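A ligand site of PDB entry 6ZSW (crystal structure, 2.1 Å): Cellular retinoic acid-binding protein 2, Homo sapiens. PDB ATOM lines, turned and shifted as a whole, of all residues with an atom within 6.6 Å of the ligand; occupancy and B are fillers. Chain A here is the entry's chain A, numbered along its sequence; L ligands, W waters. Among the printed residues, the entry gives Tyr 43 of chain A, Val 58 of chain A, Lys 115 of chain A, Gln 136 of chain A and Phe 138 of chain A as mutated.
NZ of Lys 115 is covalently linked to C4 of the ligand (1.4 Å).
An oxygen (O3) of the ligand lies within hydrogen-bond range of the side-chain hydroxyl of Tyr 43 (2.5 Å).
The indole nitrogen of Trp 113 is in hydrogen-bond range of the side-chain carboxylate of Glu 77, 3.0 Å away.
N of Thr 65 sits at hydrogen-bond distance from O of Val 58 (2.9 Å).
O of Leu 125 lies within hydrogen-bond range of N of Gln 136, 2.8 Å away.
CE1 of Phe 19 touches O3 of the ligand (3.8 Å).
CG2 of Val 58 touches C5 of the ligand, 3.3 Å away.
Val 80 touches the ligand.
Trp 113 touches the ligand.
CD2 of Leu 125 touches C11 of the ligand, at 3.4 Å.
CG of Met 127 touches C1 of the ligand, 3.7 Å away.
Gln 136 touches the ligand.
Hydrophobic or aromatic side chains that line the ligand: Phe 19, Tyr 43, Val 58, Val 80, Trp 113, Leu 125 and Met 127.
Nine residues have an atom within 4 Å of the ligand: Phe 19, Tyr 43, Val 58, Val 80, Trp 113, Lys 115, Leu 125, Met 127 and Gln 136.
The nearest printed residue that does not touch the ligand is Ile 56 (4.4 Å).
Water W1 bridges the backbone carbonyl oxygen of Gln 78 (2.6 Å) and the side-chain amide nitrogen of Gln 101 (3.0 Å).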
ATOM      1  N   PHE A  19      20.671  13.370 -28.677  1.00  0.00           N
ATOM      2  CA  PHE A  19      19.535  13.134 -27.793  1.00  0.00           C
ATOM      3  C   PHE A  19      19.326  11.637 -27.615  1.00  0.00           C
ATOM      4  O   PHE A  19      19.142  11.123 -26.510  1.00  0.00           O
ATOM      5  CB  PHE A  19      18.301  13.855 -28.344  1.00  0.00           C
ATOM      6  CG  PHE A  19      17.102  13.760 -27.441  1.00  0.00           C
ATOM      7  CD1 PHE A  19      17.157  14.230 -26.126  1.00  0.00           C
ATOM      8  CD2 PHE A  19      15.909  13.236 -27.893  1.00  0.00           C
ATOM      9  CE1 PHE A  19      16.054  14.143 -25.288  1.00  0.00           C
ATOM     10  CE2 PHE A  19      14.805  13.126 -27.045  1.00  0.00           C
ATOM     11  CZ  PHE A  19      14.879  13.587 -25.742  1.00  0.00           C
ATOM     12  N   LEU A  22      21.820  10.053 -25.233  1.00  0.00           N
ATOM     13  CA  LEU A  22      21.551  10.424 -23.838  1.00  0.00           C
ATOM     14  C   LEU A  22      20.483   9.468 -23.283  1.00  0.00           C
ATOM     15  O   LEU A  22      20.614   8.928 -22.198  1.00  0.00           O
ATOM     16  CB  LEU A  22      21.020  11.875 -23.848  1.00  0.00           C
ATOM     17  CG  LEU A  22      20.505  12.398 -22.488  1.00  0.00           C
ATOM     18  CD1 LEU A  22      21.658  12.790 -21.606  1.00  0.00           C
ATOM     19  CD2 LEU A  22      19.574  13.601 -22.654  1.00  0.00           C
ATOM     20  N   LEU A  23      19.431   9.215 -24.063  1.00  0.00           N
ATOM     21  CA  LEU A  23      18.341   8.370 -23.580  1.00  0.00           C
ATOM     22  C   LEU A  23      18.851   6.955 -23.417  1.00  0.00           C
ATOM     23  O   LEU A  23      18.405   6.206 -22.539  1.00  0.00           O
ATOM     24  CB  LEU A  23      17.172   8.401 -24.557  1.00  0.00           C
ATOM     25  CG  LEU A  23      16.510   9.779 -24.692  1.00  0.00           C
ATOM     26  CD1 LEU A  23      15.556   9.795 -25.865  1.00  0.00           C
ATOM     27  CD2 LEU A  23      15.757  10.145 -23.403  1.00  0.00           C
ATOM     28  N   TYR A  43       9.836  20.151 -29.755  1.00  0.00           N
ATOM     29  CA  TYR A  43      10.095  20.815 -28.469  1.00  0.00           C
ATOM     30  C   TYR A  43       9.886  22.334 -28.602  1.00  0.00           C
ATOM     31  O   TYR A  43      10.486  22.957 -29.464  1.00  0.00           O
ATOM     32  CB  TYR A  43      11.536  20.587 -28.006  1.00  0.00           C
ATOM     33  CG  TYR A  43      11.687  19.379 -27.124  1.00  0.00           C
ATOM     34  CD1 TYR A  43      10.891  19.216 -26.003  1.00  0.00           C
ATOM     35  CD2 TYR A  43      12.651  18.417 -27.374  1.00  0.00           C
ATOM     36  CE1 TYR A  43      11.015  18.111 -25.170  1.00  0.00           C
ATOM     37  CE2 TYR A  43      12.790  17.309 -26.548  1.00  0.00           C
ATOM     38  CZ  TYR A  43      11.970  17.152 -25.443  1.00  0.00           C
ATOM     39  OH  TYR A  43      12.107  16.074 -24.620  1.00  0.00           O
ATOM     40  N   VAL A  45       9.829  25.921 -25.913  1.00  0.00           N
ATOM     41  CA  VAL A  45      10.144  26.285 -24.547  1.00  0.00           C
ATOM     42  C   VAL A  45       9.626  27.696 -24.335  1.00  0.00           C
ATOM     43  O   VAL A  45       9.822  28.563 -25.164  1.00  0.00           O
ATOM     44  CB  VAL A  45      11.657  26.201 -24.265  1.00  0.00           C
ATOM     45  CG1 VAL A  45      11.971  26.723 -22.876  1.00  0.00           C
ATOM     46  CG2 VAL A  45      12.193  24.781 -24.398  1.00  0.00           C
ATOM     47  N   ILE A  47       9.854  30.795 -21.591  1.00  0.00           N
ATOM     48  CA  ILE A  47      10.538  31.219 -20.367  1.00  0.00           C
ATOM     49  C   ILE A  47      10.013  32.581 -19.961  1.00  0.00           C
ATOM     50  O   ILE A  47       9.965  33.483 -20.800  1.00  0.00           O
ATOM     51  CB  ILE A  47      12.043  31.321 -20.626  1.00  0.00           C
ATOM     52  CG1 ILE A  47      12.590  29.939 -21.017  1.00  0.00           C
ATOM     53  CG2 ILE A  47      12.777  31.887 -19.404  1.00  0.00           C
ATOM     54  CD1 ILE A  47      14.095  29.866 -21.156  1.00  0.00           C
ATOM     55  N   ILE A  56       9.658  28.192 -16.345  1.00  0.00           N
ATOM     56  CA  ILE A  56       9.972  27.602 -17.630  1.00  0.00           C
ATOM     57  C   ILE A  56       8.953  26.497 -17.916  1.00  0.00           C
ATOM     58  O   ILE A  56       8.730  25.599 -17.095  1.00  0.00           O
ATOM     59  CB  ILE A  56      11.409  27.044 -17.667  1.00  0.00           C
ATOM     60  CG1 ILE A  56      12.430  28.166 -17.415  1.00  0.00           C
ATOM     61  CG2 ILE A  56      11.678  26.366 -19.011  1.00  0.00           C
ATOM     62  CD1 ILE A  56      13.860  27.691 -17.191  1.00  0.00           C
ATOM     63  N   VAL A  58       8.282  23.603 -20.786  1.00  0.00           N
ATOM     64  CA  VAL A  58       8.753  22.857 -21.942  1.00  0.00           C
ATOM     65  C   VAL A  58       7.605  21.957 -22.418  1.00  0.00           C
ATOM     66  O   VAL A  58       7.006  21.244 -21.610  1.00  0.00           O
ATOM     67  CB  VAL A  58       9.960  21.957 -21.636  1.00  0.00           C
ATOM     68  CG1 VAL A  58      10.498  21.322 -22.907  1.00  0.00           C
ATOM     69  CG2 VAL A  58      11.088  22.623 -20.871  1.00  0.00           C
ATOM     70  N   THR A  65       5.477  20.445 -19.290  1.00  0.00           N
ATOM     71  CA  THR A  65       5.925  20.484 -17.895  1.00  0.00           C
ATOM     72  C   THR A  65       6.393  21.893 -17.574  1.00  0.00           C
ATOM     73  O   THR A  65       6.862  22.595 -18.467  1.00  0.00           O
ATOM     74  CB  THR A  65       7.132  19.607 -17.598  1.00  0.00           C
ATOM     75  OG1 THR A  65       8.147  20.370 -18.237  1.00  0.00           O
ATOM     76  CG2 THR A  65       7.102  18.237 -18.243  1.00  0.00           C
ATOM     77  N   ILE A  67       8.542  24.435 -14.726  1.00  0.00           N
ATOM     78  CA  ILE A  67       9.313  24.561 -13.521  1.00  0.00           C
ATOM     79  C   ILE A  67       9.411  26.022 -13.108  1.00  0.00           C
ATOM     80  O   ILE A  67       9.281  26.947 -13.926  1.00  0.00           O
ATOM     81  CB  ILE A  67      10.686  23.883 -13.636  1.00  0.00           C
ATOM     82  CG1 ILE A  67      11.640  24.676 -14.520  1.00  0.00           C
ATOM     83  CG2 ILE A  67      10.534  22.452 -14.103  1.00  0.00           C
ATOM     84  CD1 ILE A  67      12.995  24.009 -14.621  1.00  0.00           C
ATOM     85  N   GLU A  77      12.394  18.598  -9.226  1.00  0.00           N
ATOM     86  CA  GLU A  77      11.991  18.470 -10.612  1.00  0.00           C
ATOM     87  C   GLU A  77      12.174  16.995 -11.008  1.00  0.00           C
ATOM     88  O   GLU A  77      12.420  16.146 -10.152  1.00  0.00           O
ATOM     89  CB  GLU A  77      12.719  19.530 -11.465  1.00  0.00           C
ATOM     90  CG  GLU A  77      14.216  19.286 -11.711  1.00  0.00           C
ATOM     91  CD  GLU A  77      14.876  20.132 -12.816  1.00  0.00           C
ATOM     92  OE1 GLU A  77      14.157  20.575 -13.741  1.00  0.00           O
ATOM     93  OE2 GLU A  77      16.116  20.331 -12.791  1.00  0.00           O
ATOM     94  N   GLN A  78      12.034  16.685 -12.304  1.00  0.00           N
ATOM     95  CA  GLN A  78      12.355  15.356 -12.796  1.00  0.00           C
ATOM     96  C   GLN A  78      13.637  15.423 -13.650  1.00  0.00           C
ATOM     97  O   GLN A  78      13.943  16.468 -14.229  1.00  0.00           O
ATOM     98  CB  GLN A  78      11.189  14.759 -13.607  1.00  0.00           C
ATOM     99  CG  GLN A  78       9.840  14.802 -12.887  1.00  0.00           C
ATOM    100  N   THR A  79      14.357  14.294 -13.711  1.00  0.00           N
ATOM    101  CA  THR A  79      15.354  14.018 -14.725  1.00  0.00           C
ATOM    102  C   THR A  79      14.682  13.848 -16.092  1.00  0.00           C
ATOM    103  O   THR A  79      13.460  13.709 -16.195  1.00  0.00           O
ATOM    104  CB  THR A  79      16.131  12.715 -14.459  1.00  0.00           C
ATOM    105  OG1 THR A  79      15.249  11.596 -14.442  1.00  0.00           O
ATOM    106  CG2 THR A  79      16.964  12.745 -13.199  1.00  0.00           C
ATOM    107  N   VAL A  80      15.519  13.844 -17.134  1.00  0.00           N
ATOM    108  CA  VAL A  80      15.023  13.725 -18.489  1.00  0.00           C
ATOM    109  C   VAL A  80      14.177  12.458 -18.634  1.00  0.00           C
ATOM    110  O   VAL A  80      13.177  12.473 -19.355  1.00  0.00           O
ATOM    111  CB  VAL A  80      16.171  13.840 -19.528  1.00  0.00           C
ATOM    112  CG1 VAL A  80      15.754  13.270 -20.873  1.00  0.00           C
ATOM    113  CG2 VAL A  80      16.627  15.292 -19.667  1.00  0.00           C
ATOM    114  N   GLN A 101      22.026  18.058 -10.414  1.00  0.00           N
ATOM    115  CA  GLN A 101      20.884  17.277  -9.959  1.00  0.00           C
ATOM    116  C   GLN A 101      21.349  16.068  -9.142  1.00  0.00           C
ATOM    117  O   GLN A 101      22.429  15.532  -9.407  1.00  0.00           O
ATOM    118  CB  GLN A 101      20.122  16.752 -11.178  1.00  0.00           C
ATOM    119  CG  GLN A 101      19.325  17.859 -11.870  1.00  0.00           C
ATOM    120  CD  GLN A 101      18.791  17.412 -13.197  1.00  0.00           C
ATOM    121  OE1 GLN A 101      19.407  16.602 -13.881  1.00  0.00           O
ATOM    122  NE2 GLN A 101      17.642  17.966 -13.572  1.00  0.00           N
ATOM    123  N   SER A 112      23.075  16.497 -15.415  1.00  0.00           N
ATOM    124  CA  SER A 112      23.045  17.944 -15.256  1.00  0.00           C
ATOM    125  C   SER A 112      22.445  18.568 -16.510  1.00  0.00           C
ATOM    126  O   SER A 112      22.083  17.897 -17.499  1.00  0.00           O
ATOM    127  CB  SER A 112      24.405  18.506 -14.892  1.00  0.00           C
ATOM    128  OG  SER A 112      25.362  18.238 -15.899  1.00  0.00           O
ATOM    129  N   TRP A 113      22.284  19.875 -16.446  1.00  0.00           N
ATOM    130  CA  TRP A 113      21.837  20.620 -17.590  1.00  0.00           C
ATOM    131  C   TRP A 113      22.378  22.037 -17.485  1.00  0.00           C
ATOM    132  O   TRP A 113      22.715  22.495 -16.373  1.00  0.00           O
ATOM    133  CB  TRP A 113      20.318  20.566 -17.750  1.00  0.00           C
ATOM    134  CG  TRP A 113      19.447  21.130 -16.669  1.00  0.00           C
ATOM    135  CD1 TRP A 113      18.699  20.412 -15.789  1.00  0.00           C
ATOM    136  CD2 TRP A 113      19.032  22.503 -16.514  1.00  0.00           C
ATOM    137  NE1 TRP A 113      17.892  21.233 -15.038  1.00  0.00           N
ATOM    138  CE2 TRP A 113      18.083  22.528 -15.462  1.00  0.00           C
ATOM    139  CE3 TRP A 113      19.424  23.712 -17.106  1.00  0.00           C
ATOM    140  CZ2 TRP A 113      17.550  23.712 -14.983  1.00  0.00           C
ATOM    141  CZ3 TRP A 113      18.867  24.881 -16.650  1.00  0.00           C
ATOM    142  CH2 TRP A 113      17.941  24.880 -15.607  1.00  0.00           C
ATOM    143  N   THR A 114      22.494  22.686 -18.659  1.00  0.00           N
ATOM    144  CA  THR A 114      22.865  24.101 -18.759  1.00  0.00           C
ATOM    145  C   THR A 114      21.903  24.797 -19.706  1.00  0.00           C
ATOM    146  O   THR A 114      21.323  24.168 -20.594  1.00  0.00           O
ATOM    147  CB  THR A 114      24.339  24.255 -19.153  1.00  0.00           C
ATOM    148  OG1 THR A 114      24.392  24.039 -20.572  1.00  0.00           O
ATOM    149  CG2 THR A 114      25.266  23.313 -18.393  1.00  0.00           C
ATOM    150  N   LYS A 115      21.662  26.093 -19.473  1.00  0.00           N
ATOM    151  CA  LYS A 115      21.003  26.932 -20.449  1.00  0.00           C
ATOM    152  C   LYS A 115      21.881  28.155 -20.678  1.00  0.00           C
ATOM    153  O   LYS A 115      22.379  28.779 -19.707  1.00  0.00           O
ATOM    154  CB  LYS A 115      19.617  27.419 -19.967  1.00  0.00           C
ATOM    155  CG  LYS A 115      18.394  26.630 -20.473  1.00  0.00           C
ATOM    156  CD  LYS A 115      17.081  26.786 -19.618  1.00  0.00           C
ATOM    157  CE  LYS A 115      16.344  25.499 -19.292  1.00  0.00           C
ATOM    158  NZ  LYS A 115      15.472  24.965 -20.371  1.00  0.00           N
ATOM    159  N   LEU A 125      20.516  24.672 -24.854  1.00  0.00           N
ATOM    160  CA  LEU A 125      20.407  23.717 -23.768  1.00  0.00           C
ATOM    161  C   LEU A 125      21.374  22.570 -23.963  1.00  0.00           C
ATOM    162  O   LEU A 125      21.442  21.972 -25.053  1.00  0.00           O
ATOM    163  CB  LEU A 125      18.965  23.191 -23.705  1.00  0.00           C
ATOM    164  CG  LEU A 125      18.739  22.035 -22.719  1.00  0.00           C
ATOM    165  CD1 LEU A 125      18.626  22.514 -21.260  1.00  0.00           C
ATOM    166  CD2 LEU A 125      17.497  21.257 -23.120  1.00  0.00           C
ATOM    167  N   THR A 126      22.176  22.298 -22.934  1.00  0.00           N
ATOM    168  CA  THR A 126      22.885  21.024 -22.868  1.00  0.00           C
ATOM    169  C   THR A 126      22.333  20.231 -21.702  1.00  0.00           C
ATOM    170  O   THR A 126      21.869  20.785 -20.700  1.00  0.00           O
ATOM    171  CB  THR A 126      24.405  21.187 -22.815  1.00  0.00           C
ATOM    172  OG1 THR A 126      24.635  21.473 -21.442  1.00  0.00           O
ATOM    173  CG2 THR A 126      24.956  22.285 -23.720  1.00  0.00           C
ATOM    174  N   MET A 127      22.296  18.914 -21.879  1.00  0.00           N
ATOM    175  CA  MET A 127      21.804  17.971 -20.894  1.00  0.00           C
ATOM    176  C   MET A 127      22.828  16.870 -20.884  1.00  0.00           C
ATOM    177  O   MET A 127      23.237  16.389 -21.943  1.00  0.00           O
ATOM    178  CB  MET A 127      20.462  17.357 -21.286  1.00  0.00           C
ATOM    179  CG  MET A 127      19.310  18.283 -21.226  1.00  0.00           C
ATOM    180  SD  MET A 127      17.839  17.551 -22.018  1.00  0.00           S
ATOM    181  CE  MET A 127      18.293  17.609 -23.749  1.00  0.00           C
ATOM    182  N   GLN A 136      20.819  21.086 -27.635  1.00  0.00           N
ATOM    183  CA  GLN A 136      19.623  21.478 -28.346  1.00  0.00           C
ATOM    184  C   GLN A 136      19.625  22.992 -28.483  1.00  0.00           C
ATOM    185  O   GLN A 136      19.886  23.721 -27.505  1.00  0.00           O
ATOM    186  CB  GLN A 136      18.379  20.949 -27.609  1.00  0.00           C
ATOM    187  CG  GLN A 136      18.262  19.426 -27.615  1.00  0.00           C
ATOM    188  CD  GLN A 136      16.938  19.024 -27.006  1.00  0.00           C
ATOM    189  OE1 GLN A 136      16.359  19.745 -26.209  1.00  0.00           O
ATOM    190  NE2 GLN A 136      16.430  17.867 -27.393  1.00  0.00           N
ATOM    191  N   PHE A 138      17.738  26.526 -29.839  1.00  0.00           N
ATOM    192  CA  PHE A 138      16.397  27.068 -30.026  1.00  0.00           C
ATOM    193  C   PHE A 138      16.536  28.494 -30.526  1.00  0.00           C
ATOM    194  O   PHE A 138      17.544  29.125 -30.254  1.00  0.00           O
ATOM    195  CB  PHE A 138      15.657  27.087 -28.683  1.00  0.00           C
ATOM    196  CG  PHE A 138      15.437  25.746 -28.030  1.00  0.00           C
ATOM    197  CD1 PHE A 138      16.483  25.071 -27.402  1.00  0.00           C
ATOM    198  CD2 PHE A 138      14.175  25.151 -28.022  1.00  0.00           C
ATOM    199  CE1 PHE A 138      16.275  23.825 -26.806  1.00  0.00           C
ATOM    200  CE2 PHE A 138      13.975  23.924 -27.413  1.00  0.00           C
ATOM    201  CZ  PHE A 138      15.024  23.265 -26.801  1.00  0.00           C
HETATM  202  C1  LIG L   1      16.642  19.119 -18.768  1.00  0.00           C
HETATM  203  O1  LIG L   1      15.563  19.908 -19.288  1.00  0.00           O
HETATM  204  C2  LIG L   1      15.601  21.268 -19.206  1.00  0.00           C
HETATM  205  O2  LIG L   1      16.146  21.888 -18.306  1.00  0.00           O
HETATM  206  C3  LIG L   1      14.882  22.086 -20.322  1.00  0.00           C
HETATM  207  C4  LIG L   1      14.972  23.643 -20.209  1.00  0.00           C
HETATM  208  C5  LIG L   1      14.228  21.569 -21.351  1.00  0.00           C
HETATM  209  C6  LIG L   1      14.116  20.192 -21.676  1.00  0.00           C
HETATM  210  C7  LIG L   1      13.687  19.171 -20.797  1.00  0.00           C
HETATM  211  C8  LIG L   1      13.614  17.835 -21.200  1.00  0.00           C
HETATM  212  C9  LIG L   1      13.947  17.496 -22.513  1.00  0.00           C
HETATM  213  O3  LIG L   1      13.895  16.207 -22.931  1.00  0.00           O
HETATM  214  C10 LIG L   1      14.375  18.496 -23.400  1.00  0.00           C
HETATM  215  C11 LIG L   1      14.427  19.830 -23.002  1.00  0.00           C
HETATM  216  O   HOH W   1      15.747  17.497 -15.812  1.00  0.00           O
